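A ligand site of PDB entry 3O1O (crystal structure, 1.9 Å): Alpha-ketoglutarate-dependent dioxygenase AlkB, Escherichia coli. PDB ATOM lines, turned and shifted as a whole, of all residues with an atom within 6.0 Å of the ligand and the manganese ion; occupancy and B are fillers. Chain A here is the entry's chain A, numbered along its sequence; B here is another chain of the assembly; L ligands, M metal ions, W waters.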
ATOM      1  N   MET A  51      22.944  -2.200  -4.385  1.00  0.00           N
ATOM      2  CA  MET A  51      21.903  -1.754  -5.321  1.00  0.00           C
ATOM      3  C   MET A  51      21.265  -2.873  -6.147  1.00  0.00           C
ATOM      4  O   MET A  51      21.842  -3.955  -6.347  1.00  0.00           O
ATOM      5  CB  MET A  51      22.489  -0.729  -6.295  1.00  0.00           C
ATOM      6  CG  MET A  51      22.978   0.521  -5.607  1.00  0.00           C
ATOM      7  SD  MET A  51      23.829   1.647  -6.742  1.00  0.00           S
ATOM      8  CE  MET A  51      23.710   3.157  -5.751  1.00  0.00           C
ATOM      9  N   LEU A 108      15.798   2.675  -9.188  1.00  0.00           N
ATOM     10  CA  LEU A 108      17.040   2.214  -8.548  1.00  0.00           C
ATOM     11  C   LEU A 108      16.724   1.959  -7.080  1.00  0.00           C
ATOM     12  O   LEU A 108      16.213   2.849  -6.395  1.00  0.00           O
ATOM     13  CB  LEU A 108      18.138   3.270  -8.668  1.00  0.00           C
ATOM     14  CG  LEU A 108      19.452   3.034  -7.914  1.00  0.00           C
ATOM     15  CD1 LEU A 108      20.093   1.690  -8.299  1.00  0.00           C
ATOM     16  CD2 LEU A 108      20.413   4.189  -8.168  1.00  0.00           C
ATOM     17  N   ASN A 110      18.216   1.204  -3.475  1.00  0.00           N
ATOM     18  CA  ASN A 110      19.441   1.306  -2.659  1.00  0.00           C
ATOM     19  C   ASN A 110      19.232   0.717  -1.269  1.00  0.00           C
ATOM     20  O   ASN A 110      18.240   1.039  -0.616  1.00  0.00           O
ATOM     21  CB  ASN A 110      19.854   2.759  -2.482  1.00  0.00           C
ATOM     22  CG  ASN A 110      20.186   3.464  -3.784  1.00  0.00           C
ATOM     23  OD1 ASN A 110      19.841   4.633  -3.990  1.00  0.00           O
ATOM     24  ND2 ASN A 110      20.805   2.753  -4.688  1.00  0.00           N
ATOM     25  N   TYR A 112      21.078   0.455   2.465  1.00  0.00           N
ATOM     26  CA  TYR A 112      22.130   1.015   3.311  1.00  0.00           C
ATOM     27  C   TYR A 112      22.268   0.235   4.588  1.00  0.00           C
ATOM     28  O   TYR A 112      21.354   0.243   5.408  1.00  0.00           O
ATOM     29  CB  TYR A 112      21.789   2.443   3.728  1.00  0.00           C
ATOM     30  CG  TYR A 112      21.751   3.433   2.598  1.00  0.00           C
ATOM     31  CD1 TYR A 112      20.672   3.471   1.735  1.00  0.00           C
ATOM     32  CD2 TYR A 112      22.785   4.332   2.411  1.00  0.00           C
ATOM     33  CE1 TYR A 112      20.619   4.387   0.691  1.00  0.00           C
ATOM     34  CE2 TYR A 112      22.760   5.242   1.376  1.00  0.00           C
ATOM     35  CZ  TYR A 112      21.673   5.266   0.526  1.00  0.00           C
ATOM     36  OH  TYR A 112      21.654   6.167  -0.499  1.00  0.00           O
ATOM     37  N   LEU A 118      26.378   7.844   0.319  1.00  0.00           N
ATOM     38  CA  LEU A 118      26.426   8.176  -1.081  1.00  0.00           C
ATOM     39  C   LEU A 118      26.960   9.607  -1.161  1.00  0.00           C
ATOM     40  O   LEU A 118      26.261  10.576  -0.838  1.00  0.00           O
ATOM     41  CB  LEU A 118      25.032   8.067  -1.702  1.00  0.00           C
ATOM     42  CG  LEU A 118      24.885   7.537  -3.139  1.00  0.00           C
ATOM     43  CD1 LEU A 118      25.670   6.233  -3.330  1.00  0.00           C
ATOM     44  CD2 LEU A 118      23.394   7.332  -3.523  1.00  0.00           C
ATOM     45  N   HIS A 121      26.492  13.983  -5.305  1.00  0.00           N
ATOM     46  CA  HIS A 121      26.476  13.759  -6.743  1.00  0.00           C
ATOM     47  C   HIS A 121      25.241  14.412  -7.346  1.00  0.00           C
ATOM     48  O   HIS A 121      24.349  14.854  -6.628  1.00  0.00           O
ATOM     49  CB  HIS A 121      26.491  12.261  -7.081  1.00  0.00           C
ATOM     50  CG  HIS A 121      25.261  11.551  -6.629  1.00  0.00           C
ATOM     51  ND1 HIS A 121      25.089  11.119  -5.333  1.00  0.00           N
ATOM     52  CD2 HIS A 121      24.123  11.213  -7.283  1.00  0.00           C
ATOM     53  CE1 HIS A 121      23.901  10.550  -5.213  1.00  0.00           C
ATOM     54  NE2 HIS A 121      23.302  10.585  -6.383  1.00  0.00           N
ATOM     55  N   GLN A 122      25.205  14.438  -8.667  1.00  0.00           N
ATOM     56  CA  GLN A 122      24.050  14.966  -9.390  1.00  0.00           C
ATOM     57  C   GLN A 122      23.457  13.853 -10.214  1.00  0.00           C
ATOM     58  O   GLN A 122      24.198  13.048 -10.765  1.00  0.00           O
ATOM     59  CB  GLN A 122      24.475  16.052 -10.362  1.00  0.00           C
ATOM     60  CG  GLN A 122      25.109  17.280  -9.788  1.00  0.00           C
ATOM     61  CD  GLN A 122      25.617  18.190 -10.885  1.00  0.00           C
ATOM     62  OE1 GLN A 122      26.593  17.867 -11.583  1.00  0.00           O
ATOM     63  NE2 GLN A 122      24.943  19.322 -11.074  1.00  0.00           N
ATOM     64  N   ASP A 123      22.133  13.814 -10.300  1.00  0.00           N
ATOM     65  CA  ASP A 123      21.478  12.951 -11.255  1.00  0.00           C
ATOM     66  C   ASP A 123      21.368  13.755 -12.536  1.00  0.00           C
ATOM     67  O   ASP A 123      20.599  14.696 -12.607  1.00  0.00           O
ATOM     68  CB  ASP A 123      20.096  12.544 -10.771  1.00  0.00           C
ATOM     69  CG  ASP A 123      20.130  11.486  -9.701  1.00  0.00           C
ATOM     70  OD1 ASP A 123      21.092  11.460  -8.896  1.00  0.00           O
ATOM     71  OD2 ASP A 123      19.183  10.680  -9.665  1.00  0.00           O
ATOM     72  N   SER A 135      12.120  10.144  -4.791  1.00  0.00           N
ATOM     73  CA  SER A 135      13.035   9.388  -3.934  1.00  0.00           C
ATOM     74  C   SER A 135      12.330   9.023  -2.628  1.00  0.00           C
ATOM     75  O   SER A 135      12.011   9.904  -1.821  1.00  0.00           O
ATOM     76  CB  SER A 135      14.285  10.253  -3.659  1.00  0.00           C
ATOM     77  OG  SER A 135      15.291   9.510  -2.957  1.00  0.00           O
ATOM     78  N   SER A 137      12.097   6.948   1.056  1.00  0.00           N
ATOM     79  CA  SER A 137      12.940   6.431   2.132  1.00  0.00           C
ATOM     80  C   SER A 137      12.174   5.402   2.913  1.00  0.00           C
ATOM     81  O   SER A 137      11.002   5.627   3.225  1.00  0.00           O
ATOM     82  CB  SER A 137      13.350   7.541   3.131  1.00  0.00           C
ATOM     83  OG  SER A 137      14.188   8.481   2.520  1.00  0.00           O
ATOM     84  N   PHE A 144      20.132  13.369   4.708  1.00  0.00           N
ATOM     85  CA  PHE A 144      20.148  13.672   3.290  1.00  0.00           C
ATOM     86  C   PHE A 144      20.726  15.056   3.121  1.00  0.00           C
ATOM     87  O   PHE A 144      20.321  15.988   3.836  1.00  0.00           O
ATOM     88  CB  PHE A 144      18.709  13.580   2.773  1.00  0.00           C
ATOM     89  CG  PHE A 144      18.545  13.885   1.312  1.00  0.00           C
ATOM     90  CD1 PHE A 144      19.090  13.057   0.331  1.00  0.00           C
ATOM     91  CD2 PHE A 144      17.776  14.975   0.910  1.00  0.00           C
ATOM     92  CE1 PHE A 144      18.918  13.334  -1.005  1.00  0.00           C
ATOM     93  CE2 PHE A 144      17.582  15.251  -0.426  1.00  0.00           C
ATOM     94  CZ  PHE A 144      18.167  14.428  -1.393  1.00  0.00           C
ATOM     95  N   LEU A 160      15.862  12.120   6.876  1.00  0.00           N
ATOM     96  CA  LEU A 160      14.809  11.447   6.114  1.00  0.00           C
ATOM     97  C   LEU A 160      14.443  10.208   6.921  1.00  0.00           C
ATOM     98  O   LEU A 160      15.304   9.392   7.263  1.00  0.00           O
ATOM     99  CB  LEU A 160      15.284  11.054   4.718  1.00  0.00           C
ATOM    100  CG  LEU A 160      15.678  12.229   3.794  1.00  0.00           C
ATOM    101  CD1 LEU A 160      15.957  11.715   2.390  1.00  0.00           C
ATOM    102  CD2 LEU A 160      14.523  13.223   3.742  1.00  0.00           C
ATOM    103  N   TRP A 168      12.491  16.179  -6.547  1.00  0.00           N
ATOM    104  CA  TRP A 168      13.096  17.378  -7.110  1.00  0.00           C
ATOM    105  C   TRP A 168      13.028  17.372  -8.631  1.00  0.00           C
ATOM    106  O   TRP A 168      13.045  16.324  -9.274  1.00  0.00           O
ATOM    107  CB  TRP A 168      14.500  17.634  -6.547  1.00  0.00           C
ATOM    108  CG  TRP A 168      15.570  16.570  -6.751  1.00  0.00           C
ATOM    109  CD1 TRP A 168      16.565  16.589  -7.686  1.00  0.00           C
ATOM    110  CD2 TRP A 168      15.796  15.397  -5.949  1.00  0.00           C
ATOM    111  NE1 TRP A 168      17.379  15.497  -7.530  1.00  0.00           N
ATOM    112  CE2 TRP A 168      16.923  14.746  -6.483  1.00  0.00           C
ATOM    113  CE3 TRP A 168      15.139  14.834  -4.864  1.00  0.00           C
ATOM    114  CZ2 TRP A 168      17.417  13.557  -5.952  1.00  0.00           C
ATOM    115  CZ3 TRP A 168      15.620  13.640  -4.331  1.00  0.00           C
ATOM    116  CH2 TRP A 168      16.758  13.017  -4.876  1.00  0.00           C
ATOM    117  N   HIS A 177      23.335  16.269  -4.244  1.00  0.00           N
ATOM    118  CA  HIS A 177      22.664  15.698  -3.096  1.00  0.00           C
ATOM    119  C   HIS A 177      23.436  14.442  -2.713  1.00  0.00           C
ATOM    120  O   HIS A 177      24.248  13.932  -3.489  1.00  0.00           O
ATOM    121  CB  HIS A 177      21.210  15.347  -3.457  1.00  0.00           C
ATOM    122  CG  HIS A 177      21.102  14.404  -4.620  1.00  0.00           C
ATOM    123  ND1 HIS A 177      21.182  14.826  -5.934  1.00  0.00           N
ATOM    124  CD2 HIS A 177      20.956  13.057  -4.664  1.00  0.00           C
ATOM    125  CE1 HIS A 177      21.061  13.785  -6.732  1.00  0.00           C
ATOM    126  NE2 HIS A 177      20.938  12.698  -5.997  1.00  0.00           N
ATOM    127  N   GLY A 178      23.160  13.886  -1.535  1.00  0.00           N
ATOM    128  CA  GLY A 178      23.903  12.739  -1.066  1.00  0.00           C
ATOM    129  C   GLY A 178      23.345  12.280   0.257  1.00  0.00           C
ATOM    130  O   GLY A 178      22.421  12.897   0.811  1.00  0.00           O
ATOM    131  N   ILE A 179      23.888  11.178   0.736  1.00  0.00           N
ATOM    132  CA  ILE A 179      23.503  10.580   2.009  1.00  0.00           C
ATOM    133  C   ILE A 179      24.751  10.414   2.897  1.00  0.00           C
ATOM    134  O   ILE A 179      25.765   9.859   2.464  1.00  0.00           O
ATOM    135  CB  ILE A 179      22.820   9.225   1.795  1.00  0.00           C
ATOM    136  CG1 ILE A 179      21.487   9.429   1.041  1.00  0.00           C
ATOM    137  CG2 ILE A 179      22.569   8.517   3.141  1.00  0.00           C
ATOM    138  CD1 ILE A 179      20.353   9.946   1.905  1.00  0.00           C
ATOM    139  N   ARG A 194      18.450   0.761   5.882  1.00  0.00           N
ATOM    140  CA  ARG A 194      17.602   1.703   5.190  1.00  0.00           C
ATOM    141  C   ARG A 194      17.504   1.289   3.716  1.00  0.00           C
ATOM    142  O   ARG A 194      18.484   0.851   3.120  1.00  0.00           O
ATOM    143  CB  ARG A 194      18.184   3.120   5.300  1.00  0.00           C
ATOM    144  CG  ARG A 194      17.482   4.154   4.411  1.00  0.00           C
ATOM    145  CD  ARG A 194      18.072   5.538   4.570  1.00  0.00           C
ATOM    146  NE  ARG A 194      17.307   6.546   3.839  1.00  0.00           N
ATOM    147  CZ  ARG A 194      17.625   6.994   2.633  1.00  0.00           C
ATOM    148  NH1 ARG A 194      18.706   6.538   2.013  1.00  0.00           N
ATOM    149  NH2 ARG A 194      16.868   7.920   2.041  1.00  0.00           N
ATOM    150  N   ASN A 196      16.133   2.893  -0.104  1.00  0.00           N
ATOM    151  CA  ASN A 196      15.621   4.040  -0.850  1.00  0.00           C
ATOM    152  C   ASN A 196      15.206   3.589  -2.250  1.00  0.00           C
ATOM    153  O   ASN A 196      15.873   2.737  -2.863  1.00  0.00           O
ATOM    154  CB  ASN A 196      16.681   5.128  -0.909  1.00  0.00           C
ATOM    155  CG  ASN A 196      16.397   6.170  -1.986  1.00  0.00           C
ATOM    156  OD1 ASN A 196      16.764   5.986  -3.137  1.00  0.00           O
ATOM    157  ND2 ASN A 196      15.770   7.266  -1.609  1.00  0.00           N
ATOM    158  N   THR A 198      14.549   5.107  -5.879  1.00  0.00           N
ATOM    159  CA  THR A 198      14.717   6.278  -6.719  1.00  0.00           C
ATOM    160  C   THR A 198      14.143   6.083  -8.126  1.00  0.00           C
ATOM    161  O   THR A 198      14.677   5.281  -8.909  1.00  0.00           O
ATOM    162  CB  THR A 198      16.188   6.673  -6.795  1.00  0.00           C
ATOM    163  OG1 THR A 198      16.627   7.051  -5.476  1.00  0.00           O
ATOM    164  CG2 THR A 198      16.379   7.854  -7.755  1.00  0.00           C
ATOM    165  N   ARG A 200      13.064   7.367 -11.897  1.00  0.00           N
ATOM    166  CA  ARG A 200      13.492   8.330 -12.889  1.00  0.00           C
ATOM    167  C   ARG A 200      12.839   8.038 -14.226  1.00  0.00           C
ATOM    168  O   ARG A 200      12.387   6.929 -14.481  1.00  0.00           O
ATOM    169  CB  ARG A 200      15.022   8.279 -13.067  1.00  0.00           C
ATOM    170  CG  ARG A 200      15.830   8.530 -11.794  1.00  0.00           C
ATOM    171  CD  ARG A 200      17.300   8.258 -12.058  1.00  0.00           C
ATOM    172  NE  ARG A 200      18.185   8.531 -10.923  1.00  0.00           N
ATOM    173  CZ  ARG A 200      18.658   7.603 -10.088  1.00  0.00           C
ATOM    174  NH1 ARG A 200      18.330   6.327 -10.244  1.00  0.00           N
ATOM    175  NH2 ARG A 200      19.467   7.965  -9.109  1.00  0.00           N
ATOM    176  P   MFT B   8      30.168  10.960  -8.718  1.00  0.00           P
ATOM    177  N1  MFT B   8      26.466   7.802  -7.759  1.00  0.00           N
ATOM    178  C2  MFT B   8      25.227   7.129  -7.769  1.00  0.00           C
ATOM    179  O2  MFT B   8      24.985   6.245  -6.914  1.00  0.00           O
ATOM    180  N3  MFT B   8      24.292   7.416  -8.703  1.00  0.00           N
ATOM    181  C4  MFT B   8      24.536   8.361  -9.618  1.00  0.00           C
ATOM    182  O4  MFT B   8      23.685   8.657 -10.477  1.00  0.00           O
ATOM    183  C5  MFT B   8      25.813   9.093  -9.618  1.00  0.00           C
ATOM    184  C6  MFT B   8      26.738   8.768  -8.650  1.00  0.00           C
ATOM    185  C1' MFT B   8      27.429   7.516  -6.695  1.00  0.00           C
ATOM    186  O1P MFT B   8      29.917  10.278 -10.048  1.00  0.00           O
ATOM    187  C2' MFT B   8      28.809   7.053  -7.094  1.00  0.00           C
ATOM    188  C21 MFT B   8      23.015   6.693  -8.726  1.00  0.00           C
ATOM    189  O2P MFT B   8      29.399  12.187  -8.378  1.00  0.00           O
ATOM    190  C3' MFT B   8      29.644   7.573  -5.943  1.00  0.00           C
ATOM    191  O3' MFT B   8      29.386   6.645  -4.890  1.00  0.00           O
ATOM    192  C4' MFT B   8      28.993   8.891  -5.576  1.00  0.00           C
ATOM    193  O4' MFT B   8      27.638   8.763  -6.018  1.00  0.00           O
ATOM    194  C5' MFT B   8      29.654  10.092  -6.232  1.00  0.00           C
ATOM    195  O5' MFT B   8      29.897   9.814  -7.607  1.00  0.00           O
ATOM    196  C5M MFT B   8      26.062  10.151 -10.661  1.00  0.00           C
HETATM  197  C1  LIG L   1      20.308   7.939  -5.815  1.00  0.00           C
HETATM  198  O1  LIG L   1      19.901   6.746  -5.767  1.00  0.00           O
HETATM  199  O2  LIG L   1      20.760   8.475  -6.861  1.00  0.00           O
HETATM  200  C2  LIG L   1      20.254   8.692  -4.558  1.00  0.00           C
HETATM  201  O3  LIG L   1      20.632   9.843  -4.525  1.00  0.00           O
HETATM  202  C3  LIG L   1      19.741   8.005  -3.314  1.00  0.00           C
HETATM  203  C4  LIG L   1      19.382   9.053  -2.268  1.00  0.00           C
HETATM  204  C5  LIG L   1      18.829   8.395  -1.016  1.00  0.00           C
HETATM  205  O4  LIG L   1      19.182   7.220  -0.747  1.00  0.00           O
HETATM  206  O5  LIG L   1      18.024   9.037  -0.299  1.00  0.00           O
HETATM  207 MN    MN M   1      21.141  10.671  -6.689  1.00  0.00          MN
HETATM  208  O   HOH W   1      16.288  11.148  -1.107  1.00  0.00           O
HETATM  209  O   HOH W   2      17.380   9.617  -5.092  1.00  0.00           O
HETATM  210  O   HOH W   3      18.811  10.763  -7.124  1.00  0.00           O
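Water W3 bridges the side-chain carboxylate of Asp 123 (2.6 Å) and the guanidinium group of Arg 200 (3.5 Å). Water W1 bridges OG of Ser 135 and O5 of the ligand. Water W2 bridges OG1 of Thr 198 (2.7 Å) and OG of Ser 135 (3.0 Å).
NH2 of Arg 200 lies within salt-bridge range of O1 of the ligand (3.6 Å). OH of Tyr 112 is in hydrogen-bond range of O4 of the ligand (2.7 Å). The side-chain amide oxygen of Asn 110 lies close to an oxygen (O1) of the ligand, 2.8 Å away. The guanidinium group (NH2) of Arg 194 lies within salt-bridge range of an oxygen (O5) of the ligand (2.8 Å). The side-chain amide nitrogen (ND2) of Asn 196 is in hydrogen-bond range of an oxygen (O5) of the ligand (3.2 Å). O1 of the ligand lies within hydrogen-bond range of OG1 of Thr 198.
The side-chain carboxylate (OD2) of Asp 123 lies within salt-bridge range of the guanidinium group (NE) of Arg 200. N of Tyr 112 is in hydrogen-bond range of O of Arg 194, at 2.7 Å. O of Asn 110 is in hydrogen-bond range of N of Asn 196, at 2.9 Å. NH2 of Arg 194 is in hydrogen-bond range of OG of Ser 137. The side-chain amide oxygen (OD1) of Asn 196 lies within hydrogen-bond range of the side-chain hydroxyl (OG1) of Thr 198. The side-chain amide nitrogen (ND2) of Asn 196 lies within hydrogen-bond range of the side-chain hydroxyl (OG) of Ser 135, at 2.7 Å. O of Thr 198 sits at hydrogen-bond distance from N of Leu 108. The backbone NH of Ile 179 is in hydrogen-bond range of the backbone carbonyl oxygen of Leu 118 (2.9 Å).
The manganese ion is bound by NE2 of His 177 (2.2 Å), NE2 of His 121 (2.2 Å), O2 of the ligand (2.2 Å), OD1 of Asp 123 (2.3 Å), water W3 (2.4 Å) and O3 of the ligand (2.4 Å).
Arg 200 touches the manganese ion (NH2 to MN, 3.998 Å). Within 4 Å of the manganese ion: His 121, Asp 123, His 177 and Arg 200. The nearest printed residue that does not touch the manganese ion is Trp 168 (4.8 Å).
Merely in contact with the ligand: Ile 179, MFT 8 of chain B, Leu 108, Leu 118 and Ser 135. Hydrophobic or aromatic side chains that line the ligand: Leu 108, Tyr 112, Leu 118, His 121, His 177 and Ile 179. Within 4 Å of the ligand: Leu 108, Asn 110, Tyr 112, Leu 118, His 121, Asp 123, Ser 135, His 177, Ile 179, Arg 194, Asn 196, Thr 198, Arg 200 and MFT 8 of chain B.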
